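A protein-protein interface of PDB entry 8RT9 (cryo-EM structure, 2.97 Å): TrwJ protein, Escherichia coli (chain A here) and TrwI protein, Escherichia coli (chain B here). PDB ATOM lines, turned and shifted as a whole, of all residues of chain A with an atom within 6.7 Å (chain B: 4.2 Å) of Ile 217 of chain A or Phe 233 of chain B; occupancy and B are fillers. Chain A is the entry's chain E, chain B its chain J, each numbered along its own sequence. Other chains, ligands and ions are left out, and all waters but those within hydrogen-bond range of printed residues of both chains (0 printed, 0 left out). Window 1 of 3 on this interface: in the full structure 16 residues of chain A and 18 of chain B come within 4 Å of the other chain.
NH1 of Arg 213 of chain A is in salt-bridge range of OE1 of Glu 133 of chain B.
OD1 of Asn 214 of chain A lies within hydrogen-bond range of OH of Tyr 144 of chain B (2.7 Å).
Of the 9 printed residues of chain B, 4 touch a printed residue of chain A.
Hydrophobic or aromatic side chains of chain B that line the printed part of chain A: Tyr 144 and Val 239.
Hydrophobic or aromatic side chains of chain A that line the printed part of chain B: Ile 217 and Leu 218.
Along chain A the printed residues that touch a printed residue of chain B span positions 213 to 218.
Among the printed residues, 7 pairs touch across the chains.
Among the printed residues, pairs that only touch across the chains: Ile 217 of chain A with Glu 133 of chain B, Ile 217 of chain A with Tyr 144 of chain B, Ile 217 of chain A with Phe 233 of chain B, Ile 217 of chain A with Val 239 of chain B and Leu 218 of chain A with Tyr 144 of chain B.
Val 119 of chain A touches none of the printed residues of chain B.
Of the printed residues of chain B, Asn 214 of chain A touches Tyr 144.
Asn 222 of chain A touches none of the printed residues of chain B.
Printed residues of chain A within 4 Å of Glu 133 of chain B: Arg 213 and Ile 217.
Of chain A, only Ile 217 (3.97 Å) comes within 4 Å of Phe 233 of chain B.
The nearest printed residue of chain B that does not touch Asn 214 of chain A is Glu 133 of chain B (7.1 Å).
The guanidinium group (NE) of Arg 213 of chain A lies within hydrogen-bond range of the backbone carbonyl oxygen (O) of Val 119 of chain A, at 3.1 Å.
ND2 of Asn 222 of chain A is in hydrogen-bond range of O of Ile 217 of chain A (3.3 Å).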
ATOM      1  N   VAL A 119      22.169   6.126  32.934  1.00  0.00           N
ATOM      2  CA  VAL A 119      22.921   6.196  31.691  1.00  0.00           C
ATOM      3  C   VAL A 119      22.153   6.981  30.633  1.00  0.00           C
ATOM      4  O   VAL A 119      22.755   7.671  29.801  1.00  0.00           O
ATOM      5  CB  VAL A 119      23.272   4.768  31.235  1.00  0.00           C
ATOM      6  CG1 VAL A 119      23.972   4.781  29.911  1.00  0.00           C
ATOM      7  CG2 VAL A 119      24.147   4.103  32.263  1.00  0.00           C
ATOM      8  N   GLU A 212      33.560   7.856  29.314  1.00  0.00           N
ATOM      9  CA  GLU A 212      33.151   7.452  30.654  1.00  0.00           C
ATOM     10  C   GLU A 212      31.828   6.704  30.617  1.00  0.00           C
ATOM     11  O   GLU A 212      31.673   5.670  31.278  1.00  0.00           O
ATOM     12  CB  GLU A 212      33.046   8.668  31.565  1.00  0.00           C
ATOM     13  CG  GLU A 212      32.692   8.326  32.994  1.00  0.00           C
ATOM     14  CD  GLU A 212      32.614   9.549  33.886  1.00  0.00           C
ATOM     15  OE1 GLU A 212      32.674  10.679  33.357  1.00  0.00           O
ATOM     16  OE2 GLU A 212      32.486   9.380  35.116  1.00  0.00           O
ATOM     17  N   ARG A 213      30.863   7.204  29.845  1.00  0.00           N
ATOM     18  CA  ARG A 213      29.595   6.492  29.712  1.00  0.00           C
ATOM     19  C   ARG A 213      29.800   5.120  29.091  1.00  0.00           C
ATOM     20  O   ARG A 213      29.238   4.120  29.561  1.00  0.00           O
ATOM     21  CB  ARG A 213      28.616   7.310  28.879  1.00  0.00           C
ATOM     22  CG  ARG A 213      27.215   6.746  28.856  1.00  0.00           C
ATOM     23  CD  ARG A 213      26.390   7.418  27.794  1.00  0.00           C
ATOM     24  NE  ARG A 213      25.023   6.922  27.758  1.00  0.00           N
ATOM     25  CZ  ARG A 213      24.546   6.115  26.820  1.00  0.00           C
ATOM     26  NH1 ARG A 213      25.324   5.701  25.834  1.00  0.00           N
ATOM     27  NH2 ARG A 213      23.286   5.718  26.868  1.00  0.00           N
ATOM     28  N   ASN A 214      30.615   5.053  28.039  1.00  0.00           N
ATOM     29  CA  ASN A 214      30.878   3.777  27.386  1.00  0.00           C
ATOM     30  C   ASN A 214      31.506   2.788  28.355  1.00  0.00           C
ATOM     31  O   ASN A 214      31.139   1.609  28.379  1.00  0.00           O
ATOM     32  CB  ASN A 214      31.786   3.993  26.181  1.00  0.00           C
ATOM     33  CG  ASN A 214      31.855   2.790  25.290  1.00  0.00           C
ATOM     34  OD1 ASN A 214      31.150   1.812  25.502  1.00  0.00           O
ATOM     35  ND2 ASN A 214      32.713   2.849  24.283  1.00  0.00           N
ATOM     36  N   MET A 215      32.472   3.269  29.142  1.00  0.00           N
ATOM     37  CA  MET A 215      33.157   2.387  30.124  1.00  0.00           C
ATOM     38  C   MET A 215      32.138   1.911  31.163  1.00  0.00           C
ATOM     39  O   MET A 215      32.205   0.732  31.542  1.00  0.00           O
ATOM     40  CB  MET A 215      34.305   3.115  30.830  1.00  0.00           C
ATOM     41  CG  MET A 215      35.423   3.552  29.898  1.00  0.00           C
ATOM     42  SD  MET A 215      36.302   2.184  29.096  1.00  0.00           S
ATOM     43  CE  MET A 215      37.505   3.076  28.110  1.00  0.00           C
ATOM     44  N   ARG A 216      31.233   2.795  31.593  1.00  0.00           N
ATOM     45  CA  ARG A 216      30.252   2.425  32.604  1.00  0.00           C
ATOM     46  C   ARG A 216      29.302   1.353  32.093  1.00  0.00           C
ATOM     47  O   ARG A 216      28.895   0.468  32.853  1.00  0.00           O
ATOM     48  CB  ARG A 216      29.475   3.658  33.049  1.00  0.00           C
ATOM     49  CG  ARG A 216      28.741   3.482  34.352  1.00  0.00           C
ATOM     50  CD  ARG A 216      28.369   4.831  34.927  1.00  0.00           C
ATOM     51  NE  ARG A 216      29.547   5.569  35.367  1.00  0.00           N
ATOM     52  CZ  ARG A 216      29.556   6.434  36.374  1.00  0.00           C
ATOM     53  NH1 ARG A 216      30.676   7.063  36.700  1.00  0.00           N
ATOM     54  NH2 ARG A 216      28.447   6.670  37.059  1.00  0.00           N
ATOM     55  N   ILE A 217      28.920   1.418  30.819  1.00  0.00           N
ATOM     56  CA  ILE A 217      28.031   0.391  30.279  1.00  0.00           C
ATOM     57  C   ILE A 217      28.749  -0.949  30.177  1.00  0.00           C
ATOM     58  O   ILE A 217      28.192  -1.994  30.528  1.00  0.00           O
ATOM     59  CB  ILE A 217      27.463   0.831  28.922  1.00  0.00           C
ATOM     60  CG1 ILE A 217      26.443   1.944  29.108  1.00  0.00           C
ATOM     61  CG2 ILE A 217      26.819  -0.331  28.219  1.00  0.00           C
ATOM     62  CD1 ILE A 217      25.900   2.478  27.815  1.00  0.00           C
ATOM     63  N   LEU A 218      29.994  -0.945  29.715  1.00  0.00           N
ATOM     64  CA  LEU A 218      30.715  -2.175  29.419  1.00  0.00           C
ATOM     65  C   LEU A 218      31.628  -2.627  30.548  1.00  0.00           C
ATOM     66  O   LEU A 218      32.438  -3.533  30.341  1.00  0.00           O
ATOM     67  CB  LEU A 218      31.544  -2.011  28.149  1.00  0.00           C
ATOM     68  CG  LEU A 218      30.807  -1.906  26.822  1.00  0.00           C
ATOM     69  CD1 LEU A 218      31.713  -1.266  25.803  1.00  0.00           C
ATOM     70  CD2 LEU A 218      30.348  -3.264  26.350  1.00  0.00           C
ATOM     71  N   SER A 219      31.527  -2.019  31.726  1.00  0.00           N
ATOM     72  CA  SER A 219      32.436  -2.347  32.813  1.00  0.00           C
ATOM     73  C   SER A 219      32.307  -3.809  33.208  1.00  0.00           C
ATOM     74  O   SER A 219      31.204  -4.352  33.295  1.00  0.00           O
ATOM     75  CB  SER A 219      32.156  -1.460  34.021  1.00  0.00           C
ATOM     76  OG  SER A 219      33.082  -1.711  35.060  1.00  0.00           O
ATOM     77  N   SER A 220      33.447  -4.449  33.451  1.00  0.00           N
ATOM     78  CA  SER A 220      33.463  -5.834  33.891  1.00  0.00           C
ATOM     79  C   SER A 220      33.107  -5.988  35.359  1.00  0.00           C
ATOM     80  O   SER A 220      32.923  -7.117  35.819  1.00  0.00           O
ATOM     81  CB  SER A 220      34.833  -6.452  33.631  1.00  0.00           C
ATOM     82  OG  SER A 220      35.855  -5.694  34.249  1.00  0.00           O
ATOM     83  N   ASN A 222      30.322  -4.991  36.565  1.00  0.00           N
ATOM     84  CA  ASN A 222      28.886  -5.190  36.635  1.00  0.00           C
ATOM     85  C   ASN A 222      28.579  -6.643  36.955  1.00  0.00           C
ATOM     86  O   ASN A 222      29.286  -7.554  36.520  1.00  0.00           O
ATOM     87  CB  ASN A 222      28.235  -4.789  35.318  1.00  0.00           C
ATOM     88  CG  ASN A 222      28.473  -3.346  34.977  1.00  0.00           C
ATOM     89  OD1 ASN A 222      28.746  -2.531  35.851  1.00  0.00           O
ATOM     90  ND2 ASN A 222      28.371  -3.016  33.701  1.00  0.00           N
ATOM     91  N   ARG B 126      15.215  -5.087  22.134  1.00  0.00           N
ATOM     92  CA  ARG B 126      16.555  -5.029  22.713  1.00  0.00           C
ATOM     93  C   ARG B 126      17.609  -4.808  21.636  1.00  0.00           C
ATOM     94  O   ARG B 126      18.554  -4.030  21.824  1.00  0.00           O
ATOM     95  CB  ARG B 126      16.839  -6.298  23.502  1.00  0.00           C
ATOM     96  CG  ARG B 126      15.877  -6.483  24.635  1.00  0.00           C
ATOM     97  CD  ARG B 126      15.869  -5.262  25.514  1.00  0.00           C
ATOM     98  NE  ARG B 126      14.609  -5.138  26.228  1.00  0.00           N
ATOM     99  CZ  ARG B 126      13.598  -4.393  25.807  1.00  0.00           C
ATOM    100  NH1 ARG B 126      13.715  -3.699  24.689  1.00  0.00           N
ATOM    101  NH2 ARG B 126      12.477  -4.331  26.505  1.00  0.00           N
ATOM    102  N   ALA B 130      20.215  -1.647  21.205  1.00  0.00           N
ATOM    103  CA  ALA B 130      21.642  -1.790  20.934  1.00  0.00           C
ATOM    104  C   ALA B 130      22.055  -0.972  19.718  1.00  0.00           C
ATOM    105  O   ALA B 130      23.111  -0.330  19.719  1.00  0.00           O
ATOM    106  CB  ALA B 130      21.993  -3.262  20.734  1.00  0.00           C
ATOM    107  N   GLU B 133      22.287   2.639  20.704  1.00  0.00           N
ATOM    108  CA  GLU B 133      23.545   2.902  21.394  1.00  0.00           C
ATOM    109  C   GLU B 133      24.701   2.965  20.411  1.00  0.00           C
ATOM    110  O   GLU B 133      25.616   3.781  20.566  1.00  0.00           O
ATOM    111  CB  GLU B 133      23.801   1.834  22.450  1.00  0.00           C
ATOM    112  CG  GLU B 133      22.936   1.973  23.674  1.00  0.00           C
ATOM    113  CD  GLU B 133      23.182   3.273  24.403  1.00  0.00           C
ATOM    114  OE1 GLU B 133      24.350   3.706  24.467  1.00  0.00           O
ATOM    115  OE2 GLU B 133      22.208   3.865  24.910  1.00  0.00           O
ATOM    116  N   TYR B 144      28.313  -2.175  19.817  1.00  0.00           N
ATOM    117  CA  TYR B 144      26.884  -2.258  20.071  1.00  0.00           C
ATOM    118  C   TYR B 144      26.133  -2.747  18.845  1.00  0.00           C
ATOM    119  O   TYR B 144      25.111  -3.426  18.975  1.00  0.00           O
ATOM    120  CB  TYR B 144      26.358  -0.905  20.529  1.00  0.00           C
ATOM    121  CG  TYR B 144      26.977  -0.432  21.817  1.00  0.00           C
ATOM    122  CD1 TYR B 144      28.151   0.293  21.816  1.00  0.00           C
ATOM    123  CD2 TYR B 144      26.391  -0.720  23.033  1.00  0.00           C
ATOM    124  CE1 TYR B 144      28.719   0.722  22.987  1.00  0.00           C
ATOM    125  CE2 TYR B 144      26.952  -0.296  24.207  1.00  0.00           C
ATOM    126  CZ  TYR B 144      28.116   0.425  24.179  1.00  0.00           C
ATOM    127  OH  TYR B 144      28.683   0.853  25.352  1.00  0.00           O
ATOM    128  N   LEU B 231      16.124  -7.450  29.812  1.00  0.00           N
ATOM    129  CA  LEU B 231      17.474  -7.051  29.433  1.00  0.00           C
ATOM    130  C   LEU B 231      17.566  -5.541  29.276  1.00  0.00           C
ATOM    131  O   LEU B 231      16.668  -4.904  28.720  1.00  0.00           O
ATOM    132  CB  LEU B 231      17.878  -7.736  28.130  1.00  0.00           C
ATOM    133  CG  LEU B 231      19.348  -7.743  27.732  1.00  0.00           C
ATOM    134  CD1 LEU B 231      19.682  -9.050  27.064  1.00  0.00           C
ATOM    135  CD2 LEU B 231      19.660  -6.594  26.803  1.00  0.00           C
ATOM    136  N   ARG B 232      18.666  -4.968  29.763  1.00  0.00           N
ATOM    137  CA  ARG B 232      18.864  -3.524  29.750  1.00  0.00           C
ATOM    138  C   ARG B 232      20.339  -3.209  29.571  1.00  0.00           C
ATOM    139  O   ARG B 232      21.196  -3.900  30.124  1.00  0.00           O
ATOM    140  CB  ARG B 232      18.359  -2.885  31.042  1.00  0.00           C
ATOM    141  CG  ARG B 232      16.863  -2.927  31.214  1.00  0.00           C
ATOM    142  CD  ARG B 232      16.440  -2.110  32.404  1.00  0.00           C
ATOM    143  NE  ARG B 232      16.975  -2.676  33.634  1.00  0.00           N
ATOM    144  CZ  ARG B 232      16.364  -3.614  34.347  1.00  0.00           C
ATOM    145  NH1 ARG B 232      15.196  -4.093  33.949  1.00  0.00           N
ATOM    146  NH2 ARG B 232      16.922  -4.074  35.457  1.00  0.00           N
ATOM    147  N   PHE B 233      20.629  -2.170  28.797  1.00  0.00           N
ATOM    148  CA  PHE B 233      21.996  -1.667  28.660  1.00  0.00           C
ATOM    149  C   PHE B 233      22.270  -0.528  29.633  1.00  0.00           C
ATOM    150  O   PHE B 233      22.735   0.539  29.247  1.00  0.00           O
ATOM    151  CB  PHE B 233      22.250  -1.220  27.228  1.00  0.00           C
ATOM    152  CG  PHE B 233      22.414  -2.350  26.265  1.00  0.00           C
ATOM    153  CD1 PHE B 233      23.620  -3.002  26.147  1.00  0.00           C
ATOM    154  CD2 PHE B 233      21.360  -2.758  25.474  1.00  0.00           C
ATOM    155  CE1 PHE B 233      23.771  -4.039  25.264  1.00  0.00           C
ATOM    156  CE2 PHE B 233      21.508  -3.795  24.591  1.00  0.00           C
ATOM    157  CZ  PHE B 233      22.715  -4.435  24.486  1.00  0.00           C
ATOM    158  N   ASP B 234      21.979  -0.745  30.909  1.00  0.00           N
ATOM    159  CA  ASP B 234      22.263   0.248  31.927  1.00  0.00           C
ATOM    160  C   ASP B 234      23.652   0.002  32.500  1.00  0.00           C
ATOM    161  O   ASP B 234      24.402  -0.857  32.035  1.00  0.00           O
ATOM    162  CB  ASP B 234      21.201   0.220  33.019  1.00  0.00           C
ATOM    163  CG  ASP B 234      20.917  -1.179  33.518  1.00  0.00           C
ATOM    164  OD1 ASP B 234      21.562  -2.128  33.031  1.00  0.00           O
ATOM    165  OD2 ASP B 234      20.046  -1.331  34.399  1.00  0.00           O
ATOM    166  N   VAL B 239      26.932  -6.716  30.248  1.00  0.00           N
ATOM    167  CA  VAL B 239      26.517  -6.940  28.869  1.00  0.00           C
ATOM    168  C   VAL B 239      26.855  -8.357  28.437  1.00  0.00           C
ATOM    169  O   VAL B 239      26.052  -9.032  27.781  1.00  0.00           O
ATOM    170  CB  VAL B 239      27.161  -5.895  27.946  1.00  0.00           C
ATOM    171  CG1 VAL B 239      27.031  -6.318  26.505  1.00  0.00           C
ATOM    172  CG2 VAL B 239      26.516  -4.551  28.159  1.00  0.00           C
